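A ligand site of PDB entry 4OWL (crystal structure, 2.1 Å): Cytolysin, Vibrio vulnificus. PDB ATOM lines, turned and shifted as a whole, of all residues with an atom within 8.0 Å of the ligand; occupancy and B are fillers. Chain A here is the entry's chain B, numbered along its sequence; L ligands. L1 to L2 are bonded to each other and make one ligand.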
ATOM      1  N   CYS A  18       2.225 -16.187 -16.169  1.00  0.00           N
ATOM      2  CA  CYS A  18       3.661 -16.276 -15.906  1.00  0.00           C
ATOM      3  C   CYS A  18       3.895 -16.340 -14.415  1.00  0.00           C
ATOM      4  O   CYS A  18       3.134 -15.750 -13.635  1.00  0.00           O
ATOM      5  CB  CYS A  18       4.408 -15.077 -16.502  1.00  0.00           C
ATOM      6  SG  CYS A  18       4.751 -15.292 -18.296  1.00  0.00           S
ATOM      7  N   LEU A  19       4.935 -17.051 -13.995  1.00  0.00           N
ATOM      8  CA  LEU A  19       5.261 -17.112 -12.587  1.00  0.00           C
ATOM      9  C   LEU A  19       5.794 -15.746 -12.195  1.00  0.00           C
ATOM     10  O   LEU A  19       6.672 -15.197 -12.867  1.00  0.00           O
ATOM     11  CB  LEU A  19       6.258 -18.221 -12.281  1.00  0.00           C
ATOM     12  CG  LEU A  19       6.421 -18.527 -10.787  1.00  0.00           C
ATOM     13  CD1 LEU A  19       5.157 -19.162 -10.195  1.00  0.00           C
ATOM     14  CD2 LEU A  19       7.636 -19.406 -10.531  1.00  0.00           C
ATOM     15  N   ASP A  20       5.256 -15.197 -11.117  1.00  0.00           N
ATOM     16  CA  ASP A  20       5.356 -13.762 -10.849  1.00  0.00           C
ATOM     17  C   ASP A  20       5.517 -13.476  -9.355  1.00  0.00           C
ATOM     18  O   ASP A  20       4.749 -13.968  -8.532  1.00  0.00           O
ATOM     19  CB  ASP A  20       4.111 -13.058 -11.387  1.00  0.00           C
ATOM     20  CG  ASP A  20       4.138 -11.531 -11.179  1.00  0.00           C
ATOM     21  OD1 ASP A  20       4.121 -11.068 -10.004  1.00  0.00           O
ATOM     22  OD2 ASP A  20       4.121 -10.799 -12.188  1.00  0.00           O
ATOM     23  N   VAL A  21       6.501 -12.652  -9.016  1.00  0.00           N
ATOM     24  CA  VAL A  21       6.678 -12.233  -7.620  1.00  0.00           C
ATOM     25  C   VAL A  21       5.712 -11.113  -7.287  1.00  0.00           C
ATOM     26  O   VAL A  21       5.840 -10.002  -7.791  1.00  0.00           O
ATOM     27  CB  VAL A  21       8.121 -11.761  -7.352  1.00  0.00           C
ATOM     28  CG1 VAL A  21       8.304 -11.406  -5.863  1.00  0.00           C
ATOM     29  CG2 VAL A  21       9.107 -12.833  -7.800  1.00  0.00           C
ATOM     30  N   TYR A  22       4.735 -11.411  -6.435  1.00  0.00           N
ATOM     31  CA  TYR A  22       3.764 -10.395  -6.009  1.00  0.00           C
ATOM     32  C   TYR A  22       4.422  -9.375  -5.073  1.00  0.00           C
ATOM     33  O   TYR A  22       4.242  -8.156  -5.223  1.00  0.00           O
ATOM     34  CB  TYR A  22       2.570 -11.064  -5.316  1.00  0.00           C
ATOM     35  CG  TYR A  22       1.539 -11.647  -6.259  1.00  0.00           C
ATOM     36  CD1 TYR A  22       1.899 -12.060  -7.547  1.00  0.00           C
ATOM     37  CD2 TYR A  22       0.216 -11.790  -5.867  1.00  0.00           C
ATOM     38  CE1 TYR A  22       0.950 -12.590  -8.417  1.00  0.00           C
ATOM     39  CE2 TYR A  22      -0.731 -12.327  -6.716  1.00  0.00           C
ATOM     40  CZ  TYR A  22      -0.358 -12.717  -7.989  1.00  0.00           C
ATOM     41  OH  TYR A  22      -1.304 -13.251  -8.828  1.00  0.00           O
ATOM     42  N   GLY A  23       5.198  -9.885  -4.127  1.00  0.00           N
ATOM     43  CA  GLY A  23       5.833  -9.037  -3.135  1.00  0.00           C
ATOM     44  C   GLY A  23       4.900  -8.708  -1.988  1.00  0.00           C
ATOM     45  O   GLY A  23       3.841  -9.311  -1.827  1.00  0.00           O
ATOM     46  N   GLU A  24       5.320  -7.727  -1.180  1.00  0.00           N
ATOM     47  CA  GLU A  24       4.574  -7.297  -0.014  1.00  0.00           C
ATOM     48  C   GLU A  24       4.117  -5.858  -0.222  1.00  0.00           C
ATOM     49  O   GLU A  24       4.955  -4.979  -0.409  1.00  0.00           O
ATOM     50  CB  GLU A  24       5.427  -7.400   1.256  1.00  0.00           C
ATOM     51  N   ASN A  25       2.802  -5.652  -0.184  1.00  0.00           N
ATOM     52  CA  ASN A  25       2.181  -4.320  -0.281  1.00  0.00           C
ATOM     53  C   ASN A  25       2.680  -3.516  -1.479  1.00  0.00           C
ATOM     54  O   ASN A  25       2.871  -2.300  -1.386  1.00  0.00           O
ATOM     55  CB  ASN A  25       2.405  -3.524   1.016  1.00  0.00           C
ATOM     56  N   GLY A  26       2.894  -4.208  -2.603  1.00  0.00           N
ATOM     57  CA  GLY A  26       3.362  -3.582  -3.825  1.00  0.00           C
ATOM     58  C   GLY A  26       4.867  -3.670  -4.021  1.00  0.00           C
ATOM     59  O   GLY A  26       5.362  -3.544  -5.141  1.00  0.00           O
ATOM     60  N   ASP A  27       5.584  -3.893  -2.917  1.00  0.00           N
ATOM     61  CA  ASP A  27       7.034  -4.021  -2.956  1.00  0.00           C
ATOM     62  C   ASP A  27       7.481  -5.453  -3.290  1.00  0.00           C
ATOM     63  O   ASP A  27       7.327  -6.361  -2.473  1.00  0.00           O
ATOM     64  CB  ASP A  27       7.636  -3.615  -1.620  1.00  0.00           C
ATOM     65  CG  ASP A  27       9.072  -4.044  -1.476  1.00  0.00           C
ATOM     66  OD1 ASP A  27       9.959  -3.415  -2.103  1.00  0.00           O
ATOM     67  OD2 ASP A  27       9.316  -5.031  -0.753  1.00  0.00           O
ATOM     68  N   LYS A  28       8.076  -5.627  -4.467  1.00  0.00           N
ATOM     69  CA  LYS A  28       8.355  -6.969  -4.994  1.00  0.00           C
ATOM     70  C   LYS A  28       9.759  -7.527  -4.627  1.00  0.00           C
ATOM     71  O   LYS A  28      10.150  -8.584  -5.087  1.00  0.00           O
ATOM     72  CB  LYS A  28       8.185  -6.965  -6.522  1.00  0.00           C
ATOM     73  N   SER A  34       5.393 -12.902  -1.791  1.00  0.00           N
ATOM     74  CA  SER A  34       4.592 -13.969  -2.362  1.00  0.00           C
ATOM     75  C   SER A  34       4.829 -14.125  -3.868  1.00  0.00           C
ATOM     76  O   SER A  34       5.137 -13.173  -4.589  1.00  0.00           O
ATOM     77  CB  SER A  34       3.103 -13.725  -2.095  1.00  0.00           C
ATOM     78  OG  SER A  34       2.357 -14.864  -2.505  1.00  0.00           O
ATOM     79  N   VAL A  35       4.658 -15.369  -4.317  1.00  0.00           N
ATOM     80  CA  VAL A  35       4.796 -15.727  -5.721  1.00  0.00           C
ATOM     81  C   VAL A  35       3.523 -16.413  -6.175  1.00  0.00           C
ATOM     82  O   VAL A  35       3.047 -17.352  -5.518  1.00  0.00           O
ATOM     83  CB  VAL A  35       6.005 -16.669  -5.944  1.00  0.00           C
ATOM     84  CG1 VAL A  35       6.125 -17.057  -7.402  1.00  0.00           C
ATOM     85  CG2 VAL A  35       7.277 -15.993  -5.489  1.00  0.00           C
ATOM     86  N   ASN A  36       2.972 -15.907  -7.271  1.00  0.00           N
ATOM     87  CA  ASN A  36       1.785 -16.459  -7.914  1.00  0.00           C
ATOM     88  C   ASN A  36       1.800 -16.174  -9.436  1.00  0.00           C
ATOM     89  O   ASN A  36       2.875 -15.957 -10.007  1.00  0.00           O
ATOM     90  CB  ASN A  36       0.516 -15.909  -7.250  1.00  0.00           C
ATOM     91  CG  ASN A  36       0.223 -16.537  -5.905  1.00  0.00           C
ATOM     92  OD1 ASN A  36      -0.247 -17.680  -5.825  1.00  0.00           O
ATOM     93  ND2 ASN A  36       0.480 -15.794  -4.827  1.00  0.00           N
ATOM     94  N   GLY A  37       0.640 -16.204 -10.069  1.00  0.00           N
ATOM     95  CA  GLY A  37       0.537 -16.023 -11.516  1.00  0.00           C
ATOM     96  C   GLY A  37       0.045 -14.643 -11.925  1.00  0.00           C
ATOM     97  O   GLY A  37      -0.733 -14.017 -11.222  1.00  0.00           O
ATOM     98  N   TRP A  38       0.491 -14.198 -13.089  1.00  0.00           N
ATOM     99  CA  TRP A  38       0.074 -12.924 -13.671  1.00  0.00           C
ATOM    100  C   TRP A  38       0.245 -12.978 -15.188  1.00  0.00           C
ATOM    101  O   TRP A  38       1.055 -13.744 -15.714  1.00  0.00           O
ATOM    102  CB  TRP A  38       0.892 -11.781 -13.076  1.00  0.00           C
ATOM    103  CG  TRP A  38       0.225 -10.430 -13.140  1.00  0.00           C
ATOM    104  CD1 TRP A  38       0.419  -9.455 -14.077  1.00  0.00           C
ATOM    105  CD2 TRP A  38      -0.755  -9.909 -12.218  1.00  0.00           C
ATOM    106  NE1 TRP A  38      -0.363  -8.362 -13.801  1.00  0.00           N
ATOM    107  CE2 TRP A  38      -1.096  -8.622 -12.669  1.00  0.00           C
ATOM    108  CE3 TRP A  38      -1.367 -10.414 -11.074  1.00  0.00           C
ATOM    109  CZ2 TRP A  38      -2.028  -7.813 -11.992  1.00  0.00           C
ATOM    110  CZ3 TRP A  38      -2.290  -9.616 -10.397  1.00  0.00           C
ATOM    111  CH2 TRP A  38      -2.613  -8.334 -10.869  1.00  0.00           C
ATOM    112  N   SER A  39      -0.520 -12.158 -15.898  1.00  0.00           N
ATOM    113  CA  SER A  39      -0.341 -12.023 -17.330  1.00  0.00           C
ATOM    114  C   SER A  39       1.108 -11.625 -17.601  1.00  0.00           C
ATOM    115  O   SER A  39       1.705 -10.851 -16.837  1.00  0.00           O
ATOM    116  CB  SER A  39      -1.326 -11.011 -17.926  1.00  0.00           C
ATOM    117  OG  SER A  39      -1.213  -9.740 -17.290  1.00  0.00           O
ATOM    118  N   CYS A  40       1.668 -12.154 -18.675  1.00  0.00           N
ATOM    119  CA  CYS A  40       3.083 -11.967 -18.985  1.00  0.00           C
ATOM    120  C   CYS A  40       3.381 -10.558 -19.454  1.00  0.00           C
ATOM    121  O   CYS A  40       2.676 -10.023 -20.311  1.00  0.00           O
ATOM    122  CB  CYS A  40       3.519 -12.961 -20.058  1.00  0.00           C
ATOM    123  SG  CYS A  40       3.275 -14.699 -19.594  1.00  0.00           S
ATOM    124  N   HIS A  41       4.439  -9.968 -18.895  1.00  0.00           N
ATOM    125  CA  HIS A  41       4.930  -8.690 -19.383  1.00  0.00           C
ATOM    126  C   HIS A  41       6.459  -8.657 -19.420  1.00  0.00           C
ATOM    127  O   HIS A  41       7.057  -7.785 -20.038  1.00  0.00           O
ATOM    128  CB  HIS A  41       4.375  -7.516 -18.555  1.00  0.00           C
ATOM    129  CG  HIS A  41       4.399  -7.719 -17.074  1.00  0.00           C
ATOM    130  ND1 HIS A  41       5.553  -7.991 -16.372  1.00  0.00           N
ATOM    131  CD2 HIS A  41       3.410  -7.623 -16.142  1.00  0.00           C
ATOM    132  CE1 HIS A  41       5.280  -8.079 -15.082  1.00  0.00           C
ATOM    133  NE2 HIS A  41       3.988  -7.871 -14.924  1.00  0.00           N
ATOM    134  N   GLY A  42       7.101  -9.617 -18.761  1.00  0.00           N
ATOM    135  CA  GLY A  42       8.546  -9.742 -18.841  1.00  0.00           C
ATOM    136  C   GLY A  42       9.347  -8.824 -17.934  1.00  0.00           C
ATOM    137  O   GLY A  42      10.568  -9.002 -17.842  1.00  0.00           O
ATOM    138  N   SER A  43       8.701  -7.854 -17.282  1.00  0.00           N
ATOM    139  CA  SER A  43       9.369  -7.014 -16.272  1.00  0.00           C
ATOM    140  C   SER A  43      10.107  -7.884 -15.242  1.00  0.00           C
ATOM    141  O   SER A  43       9.840  -9.077 -15.126  1.00  0.00           O
ATOM    142  CB  SER A  43       8.363  -6.098 -15.577  1.00  0.00           C
ATOM    143  N   ASN A  45      10.217  -8.867 -12.208  1.00  0.00           N
ATOM    144  CA  ASN A  45       9.636  -9.793 -11.233  1.00  0.00           C
ATOM    145  C   ASN A  45       8.965 -11.024 -11.839  1.00  0.00           C
ATOM    146  O   ASN A  45       8.261 -11.767 -11.141  1.00  0.00           O
ATOM    147  CB  ASN A  45       8.598  -9.071 -10.384  1.00  0.00           C
ATOM    148  CG  ASN A  45       7.432  -8.576 -11.198  1.00  0.00           C
ATOM    149  OD1 ASN A  45       7.613  -8.105 -12.315  1.00  0.00           O
ATOM    150  ND2 ASN A  45       6.230  -8.671 -10.645  1.00  0.00           N
ATOM    151  N   GLN A  46       9.182 -11.241 -13.136  1.00  0.00           N
ATOM    152  CA  GLN A  46       8.724 -12.452 -13.824  1.00  0.00           C
ATOM    153  C   GLN A  46       9.903 -13.118 -14.516  1.00  0.00           C
ATOM    154  O   GLN A  46       9.728 -13.928 -15.458  1.00  0.00           O
ATOM    155  CB  GLN A  46       7.647 -12.124 -14.853  1.00  0.00           C
ATOM    156  CG  GLN A  46       6.314 -11.678 -14.264  1.00  0.00           C
ATOM    157  CD  GLN A  46       5.286 -11.299 -15.340  1.00  0.00           C
ATOM    158  OE1 GLN A  46       5.598 -11.224 -16.540  1.00  0.00           O
ATOM    159  NE2 GLN A  46       4.046 -11.079 -14.904  1.00  0.00           N
ATOM    160  N   ARG A 114      -5.363 -17.428 -10.698  1.00  0.00           N
ATOM    161  CA  ARG A 114      -3.979 -16.942 -10.784  1.00  0.00           C
ATOM    162  C   ARG A 114      -3.146 -17.430  -9.612  1.00  0.00           C
ATOM    163  O   ARG A 114      -1.992 -17.034  -9.459  1.00  0.00           O
ATOM    164  CB  ARG A 114      -3.949 -15.422 -10.821  1.00  0.00           C
ATOM    165  CG  ARG A 114      -4.267 -14.873 -12.189  1.00  0.00           C
ATOM    166  CD  ARG A 114      -4.009 -13.392 -12.236  1.00  0.00           C
ATOM    167  NE  ARG A 114      -3.677 -12.972 -13.597  1.00  0.00           N
ATOM    168  CZ  ARG A 114      -3.852 -11.744 -14.067  1.00  0.00           C
ATOM    169  NH1 ARG A 114      -4.364 -10.795 -13.294  1.00  0.00           N
ATOM    170  NH2 ARG A 114      -3.515 -11.466 -15.319  1.00  0.00           N
HETATM  171  C1  LIG L   1       0.151  -0.992  -8.257  1.00  0.00           C
HETATM  172  C2  LIG L   1       0.400  -2.066  -7.190  1.00  0.00           C
HETATM  173  C3  LIG L   1       1.422  -3.078  -7.695  1.00  0.00           C
HETATM  174  C4  LIG L   1       1.041  -3.601  -9.077  1.00  0.00           C
HETATM  175  C5  LIG L   1       0.667  -2.471 -10.026  1.00  0.00           C
HETATM  176  C6  LIG L   1       0.056  -2.969 -11.313  1.00  0.00           C
HETATM  177  C7  LIG L   1       0.285  -1.742  -4.747  1.00  0.00           C
HETATM  178  C8  LIG L   1       0.827  -0.969  -3.576  1.00  0.00           C
HETATM  179  N1  LIG L   1       0.821  -1.448  -5.944  1.00  0.00           N
HETATM  180  O1  LIG L   1      -0.773  -0.068  -7.819  1.00  0.00           O
HETATM  181  O2  LIG L   1       1.508  -4.192  -6.806  1.00  0.00           O
HETATM  182  O3  LIG L   1       2.121  -4.321  -9.644  1.00  0.00           O
HETATM  183  O4  LIG L   1      -0.312  -1.605  -9.427  1.00  0.00           O
HETATM  184  O5  LIG L   1      -1.092  -3.774 -11.051  1.00  0.00           O
HETATM  185  O6  LIG L   1      -0.587  -2.589  -4.613  1.00  0.00           O
HETATM  186  C1  LG2 L   2       1.686  -5.639  -9.986  1.00  0.00           C
HETATM  187  C2  LG2 L   2       2.768  -6.358 -10.810  1.00  0.00           C
HETATM  188  C3  LG2 L   2       2.231  -7.702 -11.248  1.00  0.00           C
HETATM  189  C4  LG2 L   2       1.888  -8.539  -9.990  1.00  0.00           C
HETATM  190  C5  LG2 L   2       0.873  -7.745  -9.137  1.00  0.00           C
HETATM  191  C6  LG2 L   2       0.459  -8.389  -7.786  1.00  0.00           C
HETATM  192  O1  LG2 L   2       3.167  -5.626 -11.972  1.00  0.00           O
HETATM  193  O2  LG2 L   2       3.174  -8.432 -12.043  1.00  0.00           O
HETATM  194  O3  LG2 L   2       3.075  -8.825  -9.249  1.00  0.00           O
HETATM  195  O4  LG2 L   2       1.385  -6.425  -8.826  1.00  0.00           O
HETATM  196  O5  LG2 L   2      -0.883  -8.036  -7.414  1.00  0.00           O
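The side-chain carboxylate (OD1) of Asp 20 sits at hydrogen-bond distance from the side-chain amide nitrogen (ND2) of Asn 45, 3.3 Å away.
The backbone NH (N) of His 41 sits at hydrogen-bond distance from the side-chain amide oxygen (OE1) of Gln 46 (2.9 Å).
A ring nitrogen (ND1) of His 41 lies close to the backbone NH of Ser 43 (3.3 Å).
N of Val 21 lies within hydrogen-bond range of O of Asn 45.
The backbone carbonyl oxygen (O) of Gly 37 lies within hydrogen-bond range of the side-chain hydroxyl (OH) of Tyr 22 (2.6 Å).
The backbone NH of Tyr 22 sits at hydrogen-bond distance from the backbone carbonyl oxygen of Ser 34, at 2.6 Å.
The side-chain amide oxygen of Gln 46 is in hydrogen-bond range of the backbone NH of Gly 42 (3.1 Å).
SG of Cys 18 is disulfide-bonded to SG of Cys 40 (2.1 Å).
CA of Tyr 22 touches O3 of LG2 L2 (3.7 Å).
O of Asn 25 touches C8 of LIG L1, 3.3 Å away.
Gly 26 touches the ligand.
CD1 of Trp 38 touches O2 of LG2 L2, 3.6 Å away.
Gln 46 touches the ligand.
Nine residues have an atom within 4 Å of the ligand: Asp 20, Val 21, Tyr 22, Asn 25, Gly 26, Trp 38, His 41, Asn 45 and Gln 46.
The nearest printed residue that does not touch the ligand is Ser 39 (5.6 Å).
An oxygen (O2) of LG2 L2 sits at hydrogen-bond distance from the side-chain carboxylate (OD2) of Asp 20, at 2.6 Å.
An oxygen (O2) of LG2 L2 sits at hydrogen-bond distance from a ring nitrogen (NE2) of His 41, 3.0 Å away.
The backbone carbonyl oxygen of Val 21 lies within hydrogen-bond range of an oxygen (O3) of LG2 L2 (3.3 Å).
An oxygen (O2) of LG2 L2 is in hydrogen-bond range of the side-chain amide nitrogen (ND2) of Asn 45 (3.4 Å).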
